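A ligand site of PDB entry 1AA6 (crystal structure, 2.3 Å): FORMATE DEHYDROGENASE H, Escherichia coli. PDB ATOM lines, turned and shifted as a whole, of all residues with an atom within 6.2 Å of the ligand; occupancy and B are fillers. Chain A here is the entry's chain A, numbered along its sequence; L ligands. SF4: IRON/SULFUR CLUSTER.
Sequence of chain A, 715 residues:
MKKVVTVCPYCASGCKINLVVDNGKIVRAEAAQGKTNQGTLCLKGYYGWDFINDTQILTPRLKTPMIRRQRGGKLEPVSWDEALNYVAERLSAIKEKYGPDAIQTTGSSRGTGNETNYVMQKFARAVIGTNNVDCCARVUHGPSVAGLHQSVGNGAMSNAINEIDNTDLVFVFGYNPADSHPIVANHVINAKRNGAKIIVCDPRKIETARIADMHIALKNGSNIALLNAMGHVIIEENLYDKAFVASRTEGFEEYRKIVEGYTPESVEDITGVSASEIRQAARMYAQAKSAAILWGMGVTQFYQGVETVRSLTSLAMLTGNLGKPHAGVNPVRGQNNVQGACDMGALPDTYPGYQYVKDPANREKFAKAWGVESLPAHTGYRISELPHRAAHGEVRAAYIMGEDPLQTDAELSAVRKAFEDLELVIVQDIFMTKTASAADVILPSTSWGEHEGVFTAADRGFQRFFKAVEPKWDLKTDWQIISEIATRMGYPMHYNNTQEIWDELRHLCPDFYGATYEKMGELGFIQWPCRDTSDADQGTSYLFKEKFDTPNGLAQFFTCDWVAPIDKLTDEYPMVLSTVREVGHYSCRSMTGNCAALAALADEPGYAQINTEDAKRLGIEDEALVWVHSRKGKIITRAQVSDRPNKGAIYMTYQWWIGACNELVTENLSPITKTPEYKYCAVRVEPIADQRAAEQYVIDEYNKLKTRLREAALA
Residues that only touch the ligand: Tyr 10 (3.3 Å), Gly 14 (3.9 Å), Leu 41 (3.7 Å) and Pro 182 (3.6 Å).
Hydrophobic or aromatic side chains within 4 Å of the ligand: Tyr 10, Leu 41, Pro 182 and Ile 183.
Of the 23 residues printed, 12 come within 4 Å of the ligand.
Along chain A the residues within 4 Å of the ligand span positions 8 to 183.
The nearest printed residue that does not touch the ligand is His 181 (4.5 Å).
FE3 of the ligand is bound by SG of Cys 15, at 2.2 Å.
The side-chain sulfur (SG) of Cys 8 is bound to an iron atom (FE2) of the ligand, 2.3 Å away.
N of Cys 42 sits close to S4 of the ligand, at 3.4 Å.
The side-chain sulfur (SG) of Cys 42 is bound to an iron atom (FE1) of the ligand.
The backbone NH (N) of Cys 11 sits close to a sulfur (S3) of the ligand (3.8 Å).
SG of Cys 11 binds FE4 of the ligand (2.4 Å).
The side-chain amino group (NZ) of Lys 44 sits close to a sulfur (S3) of the ligand, 3.3 Å away.
A sulfur (S2) of the ligand sits close to the side-chain hydroxyl (OG) of Ser 13, at 3.6 Å.
S2 of the ligand lies close to N of Ile 183 (3.6 Å).
The backbone NH (N) of Gly 45 lies close to a sulfur (S4) of the ligand, 3.8 Å away.
The backbone carbonyl oxygen (O) of Cys 15 is in hydrogen-bond range of the backbone NH (N) of Cys 8.
The backbone NH of Tyr 10 sits close to the side-chain sulfur of Cys 8, at 3.6 Å.
N of Lys 44 lies close to SG of Cys 42 (3.5 Å).
The side-chain sulfur (SG) of Cys 11 lies close to the side-chain hydroxyl (OG) of Ser 13.
The backbone carbonyl oxygen (O) of Ser 180 lies close to the side-chain sulfur (SG) of Cys 11 (3.5 Å).
The backbone carbonyl oxygen (O) of Tyr 10 sits at hydrogen-bond distance from the side-chain hydroxyl (OH) of Tyr 586.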
ATOM      1  N   CYS A   8      -7.284  19.769  -6.457  1.00  0.00           N
ATOM      2  CA  CYS A   8      -6.643  19.281  -5.232  1.00  0.00           C
ATOM      3  C   CYS A   8      -6.643  17.762  -5.198  1.00  0.00           C
ATOM      4  O   CYS A   8      -7.651  17.140  -5.500  1.00  0.00           O
ATOM      5  CB  CYS A   8      -7.360  19.806  -3.992  1.00  0.00           C
ATOM      6  SG  CYS A   8      -6.409  19.517  -2.458  1.00  0.00           S
ATOM      7  N   PRO A   9      -5.498  17.134  -4.855  1.00  0.00           N
ATOM      8  CA  PRO A   9      -5.428  15.680  -4.795  1.00  0.00           C
ATOM      9  C   PRO A   9      -5.601  15.151  -3.376  1.00  0.00           C
ATOM     10  O   PRO A   9      -5.123  14.076  -3.062  1.00  0.00           O
ATOM     11  CB  PRO A   9      -4.019  15.399  -5.271  1.00  0.00           C
ATOM     12  CG  PRO A   9      -3.278  16.494  -4.568  1.00  0.00           C
ATOM     13  CD  PRO A   9      -4.147  17.720  -4.751  1.00  0.00           C
ATOM     14  N   TYR A  10      -6.225  15.940  -2.502  1.00  0.00           N
ATOM     15  CA  TYR A  10      -6.417  15.484  -1.135  1.00  0.00           C
ATOM     16  C   TYR A  10      -7.774  14.910  -0.976  1.00  0.00           C
ATOM     17  O   TYR A  10      -7.985  13.763  -1.366  1.00  0.00           O
ATOM     18  CB  TYR A  10      -6.096  16.579  -0.091  1.00  0.00           C
ATOM     19  CG  TYR A  10      -4.596  16.720   0.048  1.00  0.00           C
ATOM     20  CD1 TYR A  10      -3.834  15.648   0.508  1.00  0.00           C
ATOM     21  CD2 TYR A  10      -3.923  17.832  -0.461  1.00  0.00           C
ATOM     22  CE1 TYR A  10      -2.437  15.662   0.435  1.00  0.00           C
ATOM     23  CE2 TYR A  10      -2.521  17.850  -0.542  1.00  0.00           C
ATOM     24  CZ  TYR A  10      -1.798  16.765  -0.084  1.00  0.00           C
ATOM     25  OH  TYR A  10      -0.435  16.753  -0.138  1.00  0.00           O
ATOM     26  N   CYS A  11      -8.705  15.694  -0.480  1.00  0.00           N
ATOM     27  CA  CYS A  11     -10.041  15.220  -0.271  1.00  0.00           C
ATOM     28  C   CYS A  11     -10.953  15.494  -1.460  1.00  0.00           C
ATOM     29  O   CYS A  11     -10.621  16.252  -2.394  1.00  0.00           O
ATOM     30  CB  CYS A  11     -10.604  15.784   1.045  1.00  0.00           C
ATOM     31  SG  CYS A  11     -11.454  17.400   0.980  1.00  0.00           S
ATOM     32  N   ALA A  12     -12.133  14.886  -1.414  1.00  0.00           N
ATOM     33  CA  ALA A  12     -13.106  14.959  -2.478  1.00  0.00           C
ATOM     34  C   ALA A  12     -13.845  16.248  -2.697  1.00  0.00           C
ATOM     35  O   ALA A  12     -14.765  16.264  -3.500  1.00  0.00           O
ATOM     36  CB  ALA A  12     -14.084  13.842  -2.319  1.00  0.00           C
ATOM     37  N   SER A  13     -13.473  17.325  -2.012  1.00  0.00           N
ATOM     38  CA  SER A  13     -14.147  18.628  -2.202  1.00  0.00           C
ATOM     39  C   SER A  13     -13.976  19.170  -3.614  1.00  0.00           C
ATOM     40  O   SER A  13     -14.737  20.023  -4.033  1.00  0.00           O
ATOM     41  CB  SER A  13     -13.661  19.671  -1.197  1.00  0.00           C
ATOM     42  OG  SER A  13     -13.986  19.323   0.132  1.00  0.00           O
ATOM     43  N   GLY A  14     -12.939  18.706  -4.316  1.00  0.00           N
ATOM     44  CA  GLY A  14     -12.669  19.085  -5.692  1.00  0.00           C
ATOM     45  C   GLY A  14     -12.218  20.500  -6.029  1.00  0.00           C
ATOM     46  O   GLY A  14     -12.424  20.971  -7.149  1.00  0.00           O
ATOM     47  N   CYS A  15     -11.611  21.161  -5.041  1.00  0.00           N
ATOM     48  CA  CYS A  15     -11.127  22.529  -5.172  1.00  0.00           C
ATOM     49  C   CYS A  15     -10.161  22.684  -6.353  1.00  0.00           C
ATOM     50  O   CYS A  15      -9.226  21.876  -6.514  1.00  0.00           O
ATOM     51  CB  CYS A  15     -10.386  22.948  -3.896  1.00  0.00           C
ATOM     52  SG  CYS A  15     -11.391  22.964  -2.380  1.00  0.00           S
ATOM     53  N   ILE A  17      -7.169  24.548  -8.125  1.00  0.00           N
ATOM     54  CA  ILE A  17      -5.957  25.233  -7.667  1.00  0.00           C
ATOM     55  C   ILE A  17      -5.153  25.725  -8.868  1.00  0.00           C
ATOM     56  O   ILE A  17      -5.043  25.015  -9.887  1.00  0.00           O
ATOM     57  CB  ILE A  17      -5.063  24.229  -6.916  1.00  0.00           C
ATOM     58  CG1 ILE A  17      -5.732  23.754  -5.635  1.00  0.00           C
ATOM     59  CG2 ILE A  17      -3.694  24.814  -6.637  1.00  0.00           C
ATOM     60  CD1 ILE A  17      -4.940  22.648  -4.963  1.00  0.00           C
ATOM     61  N   ASN A  37     -14.896  25.331  -4.649  1.00  0.00           N
ATOM     62  CA  ASN A  37     -14.096  26.194  -3.782  1.00  0.00           C
ATOM     63  C   ASN A  37     -14.174  27.693  -4.035  1.00  0.00           C
ATOM     64  O   ASN A  37     -13.932  28.465  -3.121  1.00  0.00           O
ATOM     65  CB  ASN A  37     -12.637  25.765  -3.783  1.00  0.00           C
ATOM     66  CG  ASN A  37     -11.986  26.002  -5.084  1.00  0.00           C
ATOM     67  OD1 ASN A  37     -12.555  25.684  -6.118  1.00  0.00           O
ATOM     68  ND2 ASN A  37     -10.790  26.579  -5.052  1.00  0.00           N
ATOM     69  N   THR A  40     -11.150  29.579  -2.576  1.00  0.00           N
ATOM     70  CA  THR A  40     -10.742  29.229  -1.226  1.00  0.00           C
ATOM     71  C   THR A  40     -10.144  27.830  -1.265  1.00  0.00           C
ATOM     72  O   THR A  40     -10.530  26.990  -2.063  1.00  0.00           O
ATOM     73  CB  THR A  40     -11.905  29.238  -0.272  1.00  0.00           C
ATOM     74  OG1 THR A  40     -12.841  28.226  -0.671  1.00  0.00           O
ATOM     75  CG2 THR A  40     -12.605  30.581  -0.320  1.00  0.00           C
ATOM     76  N   LEU A  41      -9.137  27.623  -0.437  1.00  0.00           N
ATOM     77  CA  LEU A  41      -8.458  26.345  -0.306  1.00  0.00           C
ATOM     78  C   LEU A  41      -8.199  26.247   1.156  1.00  0.00           C
ATOM     79  O   LEU A  41      -8.125  27.297   1.841  1.00  0.00           O
ATOM     80  CB  LEU A  41      -7.079  26.361  -0.967  1.00  0.00           C
ATOM     81  CG  LEU A  41      -6.849  26.387  -2.460  1.00  0.00           C
ATOM     82  CD1 LEU A  41      -5.352  26.482  -2.753  1.00  0.00           C
ATOM     83  CD2 LEU A  41      -7.429  25.140  -3.075  1.00  0.00           C
ATOM     84  N   CYS A  42      -8.031  25.029   1.648  1.00  0.00           N
ATOM     85  CA  CYS A  42      -7.708  24.824   3.062  1.00  0.00           C
ATOM     86  C   CYS A  42      -6.208  24.598   3.094  1.00  0.00           C
ATOM     87  O   CYS A  42      -5.555  24.562   2.058  1.00  0.00           O
ATOM     88  CB  CYS A  42      -8.450  23.612   3.639  1.00  0.00           C
ATOM     89  SG  CYS A  42      -7.708  21.995   3.288  1.00  0.00           S
ATOM     90  N   LEU A  43      -5.674  24.449   4.301  1.00  0.00           N
ATOM     91  CA  LEU A  43      -4.247  24.221   4.553  1.00  0.00           C
ATOM     92  C   LEU A  43      -3.563  23.196   3.609  1.00  0.00           C
ATOM     93  O   LEU A  43      -2.433  23.404   3.179  1.00  0.00           O
ATOM     94  CB  LEU A  43      -4.096  23.718   5.985  1.00  0.00           C
ATOM     95  CG  LEU A  43      -3.151  24.358   7.002  1.00  0.00           C
ATOM     96  CD1 LEU A  43      -3.377  25.837   7.126  1.00  0.00           C
ATOM     97  CD2 LEU A  43      -3.434  23.687   8.340  1.00  0.00           C
ATOM     98  N   LYS A  44      -4.256  22.127   3.271  1.00  0.00           N
ATOM     99  CA  LYS A  44      -3.665  21.081   2.422  1.00  0.00           C
ATOM    100  C   LYS A  44      -3.518  21.411   0.939  1.00  0.00           C
ATOM    101  O   LYS A  44      -2.520  21.054   0.312  1.00  0.00           O
ATOM    102  CB  LYS A  44      -4.388  19.767   2.635  1.00  0.00           C
ATOM    103  CG  LYS A  44      -4.069  19.127   3.961  1.00  0.00           C
ATOM    104  CD  LYS A  44      -5.036  18.003   4.197  1.00  0.00           C
ATOM    105  CE  LYS A  44      -6.424  18.617   4.366  1.00  0.00           C
ATOM    106  NZ  LYS A  44      -7.509  17.708   3.946  1.00  0.00           N
ATOM    107  N   GLY A  45      -4.494  22.140   0.397  1.00  0.00           N
ATOM    108  CA  GLY A  45      -4.386  22.514  -1.000  1.00  0.00           C
ATOM    109  C   GLY A  45      -3.389  23.652  -1.147  1.00  0.00           C
ATOM    110  O   GLY A  45      -2.647  23.751  -2.142  1.00  0.00           O
ATOM    111  N   TYR A  46      -3.366  24.519  -0.141  1.00  0.00           N
ATOM    112  CA  TYR A  46      -2.497  25.686  -0.116  1.00  0.00           C
ATOM    113  C   TYR A  46      -1.038  25.327   0.056  1.00  0.00           C
ATOM    114  O   TYR A  46      -0.199  25.825  -0.672  1.00  0.00           O
ATOM    115  CB  TYR A  46      -2.920  26.609   1.010  1.00  0.00           C
ATOM    116  CG  TYR A  46      -2.509  28.019   0.805  1.00  0.00           C
ATOM    117  CD1 TYR A  46      -3.328  28.892   0.099  1.00  0.00           C
ATOM    118  CD2 TYR A  46      -1.327  28.509   1.355  1.00  0.00           C
ATOM    119  CE1 TYR A  46      -2.980  30.240  -0.062  1.00  0.00           C
ATOM    120  CE2 TYR A  46      -0.954  29.869   1.228  1.00  0.00           C
ATOM    121  CZ  TYR A  46      -1.794  30.750   0.516  1.00  0.00           C
ATOM    122  OH  TYR A  46      -1.518  32.103   0.425  1.00  0.00           O
ATOM    123  N   SER A 180     -12.739  17.144   7.627  1.00  0.00           N
ATOM    124  CA  SER A 180     -12.778  16.247   6.503  1.00  0.00           C
ATOM    125  C   SER A 180     -12.870  16.818   5.119  1.00  0.00           C
ATOM    126  O   SER A 180     -12.272  16.278   4.211  1.00  0.00           O
ATOM    127  CB  SER A 180     -13.911  15.256   6.689  1.00  0.00           C
ATOM    128  OG  SER A 180     -13.365  13.985   6.938  1.00  0.00           O
ATOM    129  N   HIS A 181     -13.685  17.844   4.951  1.00  0.00           N
ATOM    130  CA  HIS A 181     -13.920  18.473   3.661  1.00  0.00           C
ATOM    131  C   HIS A 181     -14.182  19.949   3.958  1.00  0.00           C
ATOM    132  O   HIS A 181     -15.316  20.455   3.877  1.00  0.00           O
ATOM    133  CB  HIS A 181     -15.175  17.808   3.013  1.00  0.00           C
ATOM    134  CG  HIS A 181     -15.008  16.345   2.702  1.00  0.00           C
ATOM    135  ND1 HIS A 181     -15.447  15.340   3.540  1.00  0.00           N
ATOM    136  CD2 HIS A 181     -14.489  15.719   1.621  1.00  0.00           C
ATOM    137  CE1 HIS A 181     -15.188  14.167   2.997  1.00  0.00           C
ATOM    138  NE2 HIS A 181     -14.616  14.367   1.827  1.00  0.00           N
ATOM    139  N   PRO A 182     -13.126  20.686   4.306  1.00  0.00           N
ATOM    140  CA  PRO A 182     -13.224  22.122   4.634  1.00  0.00           C
ATOM    141  C   PRO A 182     -14.120  22.960   3.737  1.00  0.00           C
ATOM    142  O   PRO A 182     -14.961  23.725   4.241  1.00  0.00           O
ATOM    143  CB  PRO A 182     -11.763  22.564   4.623  1.00  0.00           C
ATOM    144  CG  PRO A 182     -11.090  21.335   5.235  1.00  0.00           C
ATOM    145  CD  PRO A 182     -11.731  20.208   4.434  1.00  0.00           C
ATOM    146  N   ILE A 183     -13.976  22.784   2.420  1.00  0.00           N
ATOM    147  CA  ILE A 183     -14.757  23.545   1.454  1.00  0.00           C
ATOM    148  C   ILE A 183     -16.232  23.162   1.470  1.00  0.00           C
ATOM    149  O   ILE A 183     -17.090  24.018   1.223  1.00  0.00           O
ATOM    150  CB  ILE A 183     -14.086  23.500   0.047  1.00  0.00           C
ATOM    151  CG1 ILE A 183     -13.133  24.711  -0.115  1.00  0.00           C
ATOM    152  CG2 ILE A 183     -15.105  23.551  -1.055  1.00  0.00           C
ATOM    153  CD1 ILE A 183     -12.149  24.911   1.053  1.00  0.00           C
ATOM    154  N   VAL A 184     -16.525  21.902   1.805  1.00  0.00           N
ATOM    155  CA  VAL A 184     -17.909  21.454   1.902  1.00  0.00           C
ATOM    156  C   VAL A 184     -18.487  22.031   3.219  1.00  0.00           C
ATOM    157  O   VAL A 184     -19.674  22.360   3.281  1.00  0.00           O
ATOM    158  CB  VAL A 184     -18.079  19.906   1.896  1.00  0.00           C
ATOM    159  CG1 VAL A 184     -19.553  19.541   1.911  1.00  0.00           C
ATOM    160  CG2 VAL A 184     -17.445  19.313   0.675  1.00  0.00           C
ATOM    161  N   TYR A 586      -2.940  14.240   5.982  1.00  0.00           N
ATOM    162  CA  TYR A 586      -3.827  13.458   5.174  1.00  0.00           C
ATOM    163  C   TYR A 586      -3.541  11.941   5.069  1.00  0.00           C
ATOM    164  O   TYR A 586      -2.490  11.532   4.590  1.00  0.00           O
ATOM    165  CB  TYR A 586      -3.914  14.080   3.787  1.00  0.00           C
ATOM    166  CG  TYR A 586      -5.063  13.546   2.980  1.00  0.00           C
ATOM    167  CD1 TYR A 586      -4.925  12.393   2.233  1.00  0.00           C
ATOM    168  CD2 TYR A 586      -6.308  14.163   3.030  1.00  0.00           C
ATOM    169  CE1 TYR A 586      -5.999  11.833   1.564  1.00  0.00           C
ATOM    170  CE2 TYR A 586      -7.394  13.621   2.353  1.00  0.00           C
ATOM    171  CZ  TYR A 586      -7.231  12.450   1.634  1.00  0.00           C
ATOM    172  OH  TYR A 586      -8.310  11.866   1.023  1.00  0.00           O
HETATM  173 FE1  SF4 L   1      -8.690  21.289   1.332  1.00  0.00          FE
HETATM  174 FE2  SF4 L   1      -8.026  20.193  -1.035  1.00  0.00          FE
HETATM  175 FE3  SF4 L   1     -10.200  21.650  -1.033  1.00  0.00          FE
HETATM  176 FE4  SF4 L   1     -10.096  19.205   0.306  1.00  0.00          FE
HETATM  177  S1  SF4 L   1      -9.958  19.512  -1.957  1.00  0.00           S
HETATM  178  S2  SF4 L   1     -11.005  21.182   1.049  1.00  0.00           S
HETATM  179  S3  SF4 L   1      -7.931  19.102   0.998  1.00  0.00           S
HETATM  180  S4  SF4 L   1      -8.107  22.511  -0.598  1.00  0.00           S
